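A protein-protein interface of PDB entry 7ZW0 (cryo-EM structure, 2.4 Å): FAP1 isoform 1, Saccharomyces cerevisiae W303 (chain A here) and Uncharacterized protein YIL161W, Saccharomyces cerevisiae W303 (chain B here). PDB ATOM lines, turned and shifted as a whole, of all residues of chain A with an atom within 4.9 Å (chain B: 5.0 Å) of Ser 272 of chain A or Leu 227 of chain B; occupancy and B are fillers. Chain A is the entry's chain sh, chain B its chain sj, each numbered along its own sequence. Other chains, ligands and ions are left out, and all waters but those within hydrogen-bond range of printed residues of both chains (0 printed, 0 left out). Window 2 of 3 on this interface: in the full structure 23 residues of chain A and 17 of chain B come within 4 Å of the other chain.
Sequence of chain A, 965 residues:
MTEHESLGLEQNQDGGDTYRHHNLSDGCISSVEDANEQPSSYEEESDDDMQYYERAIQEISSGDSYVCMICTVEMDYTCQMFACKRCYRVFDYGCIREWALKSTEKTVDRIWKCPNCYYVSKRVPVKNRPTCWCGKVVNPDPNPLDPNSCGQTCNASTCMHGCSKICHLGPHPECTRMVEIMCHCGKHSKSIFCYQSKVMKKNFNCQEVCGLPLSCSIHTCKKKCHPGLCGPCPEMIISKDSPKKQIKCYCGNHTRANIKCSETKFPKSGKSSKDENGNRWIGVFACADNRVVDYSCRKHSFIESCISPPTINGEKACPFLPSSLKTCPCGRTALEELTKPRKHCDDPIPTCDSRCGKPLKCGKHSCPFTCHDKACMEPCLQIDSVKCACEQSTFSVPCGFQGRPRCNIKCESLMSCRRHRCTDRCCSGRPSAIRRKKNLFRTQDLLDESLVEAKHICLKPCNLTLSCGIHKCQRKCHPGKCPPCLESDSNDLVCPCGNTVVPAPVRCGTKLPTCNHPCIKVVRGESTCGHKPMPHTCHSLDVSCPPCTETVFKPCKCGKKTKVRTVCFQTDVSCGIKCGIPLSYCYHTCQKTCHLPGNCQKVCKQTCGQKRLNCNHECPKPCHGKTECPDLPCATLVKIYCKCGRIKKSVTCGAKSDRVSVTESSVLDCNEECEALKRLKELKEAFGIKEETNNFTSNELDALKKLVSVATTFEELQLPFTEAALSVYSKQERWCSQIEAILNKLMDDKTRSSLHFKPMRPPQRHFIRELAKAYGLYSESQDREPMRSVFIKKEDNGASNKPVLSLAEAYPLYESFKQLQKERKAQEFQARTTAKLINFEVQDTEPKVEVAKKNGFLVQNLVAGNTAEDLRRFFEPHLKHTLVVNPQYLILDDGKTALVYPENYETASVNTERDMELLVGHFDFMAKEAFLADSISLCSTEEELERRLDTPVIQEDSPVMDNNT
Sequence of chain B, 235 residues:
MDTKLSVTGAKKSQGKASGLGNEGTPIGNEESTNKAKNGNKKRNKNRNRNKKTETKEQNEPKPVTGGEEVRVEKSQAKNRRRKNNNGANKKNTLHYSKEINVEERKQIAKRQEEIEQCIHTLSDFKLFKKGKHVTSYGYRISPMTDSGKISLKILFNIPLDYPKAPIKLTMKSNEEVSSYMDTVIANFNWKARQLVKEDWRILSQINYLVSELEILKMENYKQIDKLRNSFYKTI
Pro 267 of chain A touches Arg 228 of chain B (CD to NH2, 3.6 Å). Gly 270 of chain A touches Leu 227 of chain B. CD2 of Leu 227 of chain B touches N of Lys 271 of chain A, 3.9 Å away. CD1 of Leu 227 of chain B touches OG of Ser 272 of chain A, 3.9 Å away. Ile 282 of chain A touches Arg 228 of chain B. Phe 231 of chain B touches Ile 282 of chain A (CD1 to CB, 3.5 Å).
Printed residues of chain B within 4 Å of Gly 270 of chain A: Leu 227. Of chain B, only Leu 227 (3.9 Å) comes within 4 Å of Ser 272 of chain A. Lys 226 of chain B touches none of the printed residues of chain A. Leu 227 of chain B touches three residues of chain A. Of the printed residues of chain A, Phe 231 of chain B touches Ile 282 (3.5 Å). The nearest printed residue of chain B that does not touch Ser 272 of chain A is Ser 230 of chain B (6.5 Å). The nearest residue of chain A that does not touch Leu 227 of chain B is Ile 282 of chain A (4.3 Å).
The side-chain hydroxyl of Ser 272 of chain A is in hydrogen-bond range of the guanidinium group of Arg 280 of chain A (3.0 Å). O of Leu 227 of chain B is in hydrogen-bond range of OG of Ser 230 of chain B. O of Ile 224 of chain B sits close to NH1 of Arg 228 of chain B (3.5 Å).
Printed residues of chain A that touch a printed residue of chain B: Pro 267, Gly 270, Lys 271, Ser 272 and Ile 282. Hydrophobic or aromatic side chains of chain A that line the printed part of chain B: Pro 267 and Ile 282. Of the 10 printed residues of chain B, 3 touch a printed residue of chain A. Hydrophobic or aromatic side chains of chain B that line the printed part of chain A: Leu 227 and Phe 231. Along chain B the printed residues that touch a printed residue of chain A span positions 227 to 231. Among the printed residues, 6 pairs touch across the chains.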
ATOM      1  N   PRO A 267       8.879 -14.522 -19.843  1.00  0.00           N
ATOM      2  CA  PRO A 267       7.531 -14.907 -20.284  1.00  0.00           C
ATOM      3  C   PRO A 267       6.718 -15.619 -19.217  1.00  0.00           C
ATOM      4  O   PRO A 267       7.271 -16.407 -18.449  1.00  0.00           O
ATOM      5  CB  PRO A 267       7.798 -15.863 -21.460  1.00  0.00           C
ATOM      6  CG  PRO A 267       9.222 -15.657 -21.841  1.00  0.00           C
ATOM      7  CD  PRO A 267       9.937 -15.198 -20.609  1.00  0.00           C
ATOM      8  N   GLY A 270       6.954 -18.956 -19.750  1.00  0.00           N
ATOM      9  CA  GLY A 270       8.194 -19.497 -19.237  1.00  0.00           C
ATOM     10  C   GLY A 270       8.905 -20.215 -20.346  1.00  0.00           C
ATOM     11  O   GLY A 270       9.770 -21.055 -20.100  1.00  0.00           O
ATOM     12  N   LYS A 271       8.520 -19.910 -21.578  1.00  0.00           N
ATOM     13  CA  LYS A 271       9.173 -20.523 -22.724  1.00  0.00           C
ATOM     14  C   LYS A 271       9.888 -19.489 -23.567  1.00  0.00           C
ATOM     15  O   LYS A 271       9.390 -18.389 -23.779  1.00  0.00           O
ATOM     16  CB  LYS A 271       8.192 -21.344 -23.561  1.00  0.00           C
ATOM     17  CG  LYS A 271       7.773 -22.653 -22.917  1.00  0.00           C
ATOM     18  CD  LYS A 271       6.984 -23.515 -23.888  1.00  0.00           C
ATOM     19  CE  LYS A 271       6.636 -24.861 -23.272  1.00  0.00           C
ATOM     20  NZ  LYS A 271       5.876 -25.722 -24.219  1.00  0.00           N
ATOM     21  N   SER A 272      11.075 -19.838 -24.026  1.00  0.00           N
ATOM     22  CA  SER A 272      11.860 -18.908 -24.804  1.00  0.00           C
ATOM     23  C   SER A 272      11.283 -18.679 -26.182  1.00  0.00           C
ATOM     24  O   SER A 272      10.544 -19.512 -26.708  1.00  0.00           O
ATOM     25  CB  SER A 272      13.288 -19.414 -24.908  1.00  0.00           C
ATOM     26  OG  SER A 272      13.497 -20.526 -24.059  1.00  0.00           O
ATOM     27  N   SER A 273      11.626 -17.546 -26.773  1.00  0.00           N
ATOM     28  CA  SER A 273      11.087 -17.218 -28.066  1.00  0.00           C
ATOM     29  C   SER A 273      11.478 -18.289 -29.022  1.00  0.00           C
ATOM     30  O   SER A 273      12.652 -18.623 -29.135  1.00  0.00           O
ATOM     31  CB  SER A 273      11.745 -15.944 -28.548  1.00  0.00           C
ATOM     32  OG  SER A 273      12.187 -15.177 -27.449  1.00  0.00           O
ATOM     33  N   LYS A 274      10.505 -18.796 -29.762  1.00  0.00           N
ATOM     34  CA  LYS A 274      10.820 -19.796 -30.761  1.00  0.00           C
ATOM     35  C   LYS A 274      10.365 -19.398 -32.146  1.00  0.00           C
ATOM     36  O   LYS A 274       9.214 -19.005 -32.347  1.00  0.00           O
ATOM     37  CB  LYS A 274      10.280 -21.176 -30.363  1.00  0.00           C
ATOM     38  CG  LYS A 274       8.780 -21.261 -30.148  1.00  0.00           C
ATOM     39  CD  LYS A 274       8.160 -22.268 -31.103  1.00  0.00           C
ATOM     40  CE  LYS A 274       6.687 -22.481 -30.801  1.00  0.00           C
ATOM     41  NZ  LYS A 274       6.065 -23.442 -31.750  1.00  0.00           N
ATOM     42  N   ARG A 280      15.488 -21.731 -29.201  1.00  0.00           N
ATOM     43  CA  ARG A 280      14.847 -20.896 -28.208  1.00  0.00           C
ATOM     44  C   ARG A 280      15.808 -19.934 -27.554  1.00  0.00           C
ATOM     45  O   ARG A 280      16.759 -20.344 -26.894  1.00  0.00           O
ATOM     46  CB  ARG A 280      14.135 -21.762 -27.173  1.00  0.00           C
ATOM     47  CG  ARG A 280      12.813 -22.323 -27.668  1.00  0.00           C
ATOM     48  CD  ARG A 280      12.216 -23.313 -26.684  1.00  0.00           C
ATOM     49  NE  ARG A 280      11.984 -22.716 -25.376  1.00  0.00           N
ATOM     50  CZ  ARG A 280      11.437 -23.357 -24.349  1.00  0.00           C
ATOM     51  NH1 ARG A 280      11.061 -24.622 -24.479  1.00  0.00           N
ATOM     52  NH2 ARG A 280      11.264 -22.735 -23.192  1.00  0.00           N
ATOM     53  N   TRP A 281      15.550 -18.646 -27.725  1.00  0.00           N
ATOM     54  CA  TRP A 281      16.377 -17.640 -27.090  1.00  0.00           C
ATOM     55  C   TRP A 281      15.410 -16.957 -26.163  1.00  0.00           C
ATOM     56  O   TRP A 281      14.290 -16.647 -26.552  1.00  0.00           O
ATOM     57  CB  TRP A 281      16.974 -16.662 -28.112  1.00  0.00           C
ATOM     58  CG  TRP A 281      15.964 -15.982 -28.982  1.00  0.00           C
ATOM     59  CD1 TRP A 281      15.349 -14.791 -28.745  1.00  0.00           C
ATOM     60  CD2 TRP A 281      15.452 -16.456 -30.231  1.00  0.00           C
ATOM     61  NE1 TRP A 281      14.481 -14.496 -29.764  1.00  0.00           N
ATOM     62  CE2 TRP A 281      14.528 -15.501 -30.692  1.00  0.00           C
ATOM     63  CE3 TRP A 281      15.687 -17.595 -31.005  1.00  0.00           C
ATOM     64  CZ2 TRP A 281      13.838 -15.650 -31.888  1.00  0.00           C
ATOM     65  CZ3 TRP A 281      15.001 -17.739 -32.190  1.00  0.00           C
ATOM     66  CH2 TRP A 281      14.087 -16.773 -32.620  1.00  0.00           C
ATOM     67  N   ILE A 282      15.800 -16.766 -24.915  1.00  0.00           N
ATOM     68  CA  ILE A 282      14.860 -16.204 -23.964  1.00  0.00           C
ATOM     69  C   ILE A 282      14.471 -14.795 -24.391  1.00  0.00           C
ATOM     70  O   ILE A 282      15.334 -13.985 -24.730  1.00  0.00           O
ATOM     71  CB  ILE A 282      15.439 -16.212 -22.532  1.00  0.00           C
ATOM     72  CG1 ILE A 282      15.946 -17.608 -22.154  1.00  0.00           C
ATOM     73  CG2 ILE A 282      14.402 -15.733 -21.527  1.00  0.00           C
ATOM     74  CD1 ILE A 282      17.417 -17.855 -22.415  1.00  0.00           C
ATOM     75  N   GLY A 283      13.178 -14.498 -24.374  1.00  0.00           N
ATOM     76  CA  GLY A 283      12.719 -13.166 -24.712  1.00  0.00           C
ATOM     77  C   GLY A 283      12.204 -12.570 -23.427  1.00  0.00           C
ATOM     78  O   GLY A 283      11.563 -13.265 -22.649  1.00  0.00           O
ATOM     79  N   PRO A 309       6.300 -17.651 -27.398  1.00  0.00           N
ATOM     80  CA  PRO A 309       6.468 -18.808 -28.281  1.00  0.00           C
ATOM     81  C   PRO A 309       5.404 -18.932 -29.409  1.00  0.00           C
ATOM     82  O   PRO A 309       4.707 -19.947 -29.436  1.00  0.00           O
ATOM     83  CB  PRO A 309       6.476 -19.967 -27.297  1.00  0.00           C
ATOM     84  CG  PRO A 309       7.099 -19.355 -26.059  1.00  0.00           C
ATOM     85  CD  PRO A 309       7.172 -17.848 -26.236  1.00  0.00           C
ATOM     86  N   GLN B 223      10.210 -24.185 -12.940  1.00  0.00           N
ATOM     87  CA  GLN B 223      10.636 -24.112 -14.334  1.00  0.00           C
ATOM     88  C   GLN B 223      10.950 -22.677 -14.739  1.00  0.00           C
ATOM     89  O   GLN B 223      11.892 -22.434 -15.506  1.00  0.00           O
ATOM     90  CB  GLN B 223       9.562 -24.705 -15.247  1.00  0.00           C
ATOM     91  CG  GLN B 223       9.292 -26.189 -15.027  1.00  0.00           C
ATOM     92  CD  GLN B 223       8.251 -26.448 -13.952  1.00  0.00           C
ATOM     93  OE1 GLN B 223       7.775 -25.522 -13.295  1.00  0.00           O
ATOM     94  NE2 GLN B 223       7.893 -27.714 -13.768  1.00  0.00           N
ATOM     95  N   ILE B 224      10.179 -21.714 -14.220  1.00  0.00           N
ATOM     96  CA  ILE B 224      10.441 -20.305 -14.505  1.00  0.00           C
ATOM     97  C   ILE B 224      11.808 -19.894 -13.970  1.00  0.00           C
ATOM     98  O   ILE B 224      12.598 -19.264 -14.679  1.00  0.00           O
ATOM     99  CB  ILE B 224       9.311 -19.428 -13.929  1.00  0.00           C
ATOM    100  CG1 ILE B 224       8.069 -19.511 -14.819  1.00  0.00           C
ATOM    101  CG2 ILE B 224       9.757 -17.979 -13.779  1.00  0.00           C
ATOM    102  CD1 ILE B 224       6.883 -18.746 -14.281  1.00  0.00           C
ATOM    103  N   ASP B 225      12.126 -20.285 -12.733  1.00  0.00           N
ATOM    104  CA  ASP B 225      13.403 -19.924 -12.127  1.00  0.00           C
ATOM    105  C   ASP B 225      14.564 -20.641 -12.804  1.00  0.00           C
ATOM    106  O   ASP B 225      15.665 -20.088 -12.910  1.00  0.00           O
ATOM    107  CB  ASP B 225      13.376 -20.239 -10.631  1.00  0.00           C
ATOM    108  CG  ASP B 225      14.621 -19.762  -9.913  1.00  0.00           C
ATOM    109  OD1 ASP B 225      14.698 -18.559  -9.588  1.00  0.00           O
ATOM    110  OD2 ASP B 225      15.522 -20.592  -9.669  1.00  0.00           O
ATOM    111  N   LYS B 226      14.338 -21.875 -13.269  1.00  0.00           N
ATOM    112  CA  LYS B 226      15.349 -22.556 -14.072  1.00  0.00           C
ATOM    113  C   LYS B 226      15.612 -21.806 -15.372  1.00  0.00           C
ATOM    114  O   LYS B 226      16.768 -21.665 -15.799  1.00  0.00           O
ATOM    115  CB  LYS B 226      14.913 -23.992 -14.358  1.00  0.00           C
ATOM    116  CG  LYS B 226      15.950 -24.821 -15.099  1.00  0.00           C
ATOM    117  CD  LYS B 226      15.434 -26.221 -15.391  1.00  0.00           C
ATOM    118  CE  LYS B 226      16.456 -27.034 -16.172  1.00  0.00           C
ATOM    119  NZ  LYS B 226      15.957 -28.401 -16.490  1.00  0.00           N
ATOM    120  N   LEU B 227      14.551 -21.300 -16.005  1.00  0.00           N
ATOM    121  CA  LEU B 227      14.717 -20.511 -17.222  1.00  0.00           C
ATOM    122  C   LEU B 227      15.435 -19.197 -16.933  1.00  0.00           C
ATOM    123  O   LEU B 227      16.233 -18.724 -17.750  1.00  0.00           O
ATOM    124  CB  LEU B 227      13.357 -20.258 -17.873  1.00  0.00           C
ATOM    125  CG  LEU B 227      13.412 -19.799 -19.330  1.00  0.00           C
ATOM    126  CD1 LEU B 227      14.046 -20.876 -20.195  1.00  0.00           C
ATOM    127  CD2 LEU B 227      12.024 -19.460 -19.841  1.00  0.00           C
ATOM    128  N   ARG B 228      15.166 -18.593 -15.772  1.00  0.00           N
ATOM    129  CA  ARG B 228      15.867 -17.367 -15.389  1.00  0.00           C
ATOM    130  C   ARG B 228      17.349 -17.628 -15.162  1.00  0.00           C
ATOM    131  O   ARG B 228      18.198 -16.817 -15.548  1.00  0.00           O
ATOM    132  CB  ARG B 228      15.247 -16.745 -14.135  1.00  0.00           C
ATOM    133  CG  ARG B 228      13.765 -16.402 -14.206  1.00  0.00           C
ATOM    134  CD  ARG B 228      13.446 -15.225 -15.117  1.00  0.00           C
ATOM    135  NE  ARG B 228      13.442 -15.571 -16.533  1.00  0.00           N
ATOM    136  CZ  ARG B 228      12.463 -16.214 -17.156  1.00  0.00           C
ATOM    137  NH1 ARG B 228      11.375 -16.610 -16.515  1.00  0.00           N
ATOM    138  NH2 ARG B 228      12.573 -16.454 -18.459  1.00  0.00           N
ATOM    139  N   ASN B 229      17.672 -18.749 -14.514  1.00  0.00           N
ATOM    140  CA  ASN B 229      19.070 -19.109 -14.302  1.00  0.00           C
ATOM    141  C   ASN B 229      19.779 -19.351 -15.627  1.00  0.00           C
ATOM    142  O   ASN B 229      20.903 -18.874 -15.833  1.00  0.00           O
ATOM    143  CB  ASN B 229      19.160 -20.347 -13.410  1.00  0.00           C
ATOM    144  CG  ASN B 229      18.749 -20.062 -11.979  1.00  0.00           C
ATOM    145  OD1 ASN B 229      19.103 -19.028 -11.414  1.00  0.00           O
ATOM    146  ND2 ASN B 229      17.994 -20.980 -11.387  1.00  0.00           N
ATOM    147  N   SER B 230      19.119 -20.056 -16.552  1.00  0.00           N
ATOM    148  CA  SER B 230      19.693 -20.276 -17.877  1.00  0.00           C
ATOM    149  C   SER B 230      19.879 -18.963 -18.630  1.00  0.00           C
ATOM    150  O   SER B 230      20.901 -18.764 -19.296  1.00  0.00           O
ATOM    151  CB  SER B 230      18.809 -21.232 -18.677  1.00  0.00           C
ATOM    152  OG  SER B 230      17.572 -20.625 -19.004  1.00  0.00           O
ATOM    153  N   PHE B 231      18.911 -18.052 -18.518  1.00  0.00           N
ATOM    154  CA  PHE B 231      18.994 -16.752 -19.178  1.00  0.00           C
ATOM    155  C   PHE B 231      20.164 -15.934 -18.637  1.00  0.00           C
ATOM    156  O   PHE B 231      20.995 -15.425 -19.404  1.00  0.00           O
ATOM    157  CB  PHE B 231      17.662 -16.023 -18.983  1.00  0.00           C
ATOM    158  CG  PHE B 231      17.659 -14.591 -19.431  1.00  0.00           C
ATOM    159  CD1 PHE B 231      17.793 -14.267 -20.772  1.00  0.00           C
ATOM    160  CD2 PHE B 231      17.478 -13.569 -18.513  1.00  0.00           C
ATOM    161  CE1 PHE B 231      17.765 -12.949 -21.187  1.00  0.00           C
ATOM    162  CE2 PHE B 231      17.453 -12.248 -18.921  1.00  0.00           C
ATOM    163  CZ  PHE B 231      17.593 -11.937 -20.259  1.00  0.00           C
ATOM    164  N   TYR B 232      20.268 -15.844 -17.311  1.00  0.00           N
ATOM    165  CA  TYR B 232      21.344 -15.083 -16.689  1.00  0.00           C
ATOM    166  C   TYR B 232      22.706 -15.730 -16.896  1.00  0.00           C
ATOM    167  O   TYR B 232      23.726 -15.040 -16.790  1.00  0.00           O
ATOM    168  CB  TYR B 232      21.052 -14.899 -15.200  1.00  0.00           C
ATOM    169  CG  TYR B 232      19.909 -13.943 -14.936  1.00  0.00           C
ATOM    170  CD1 TYR B 232      19.779 -12.771 -15.671  1.00  0.00           C
ATOM    171  CD2 TYR B 232      18.959 -14.215 -13.961  1.00  0.00           C
ATOM    172  CE1 TYR B 232      18.737 -11.894 -15.439  1.00  0.00           C
ATOM    173  CE2 TYR B 232      17.911 -13.343 -13.721  1.00  0.00           C
ATOM    174  CZ  TYR B 232      17.806 -12.184 -14.464  1.00  0.00           C
ATOM    175  OH  TYR B 232      16.767 -11.314 -14.229  1.00  0.00           O
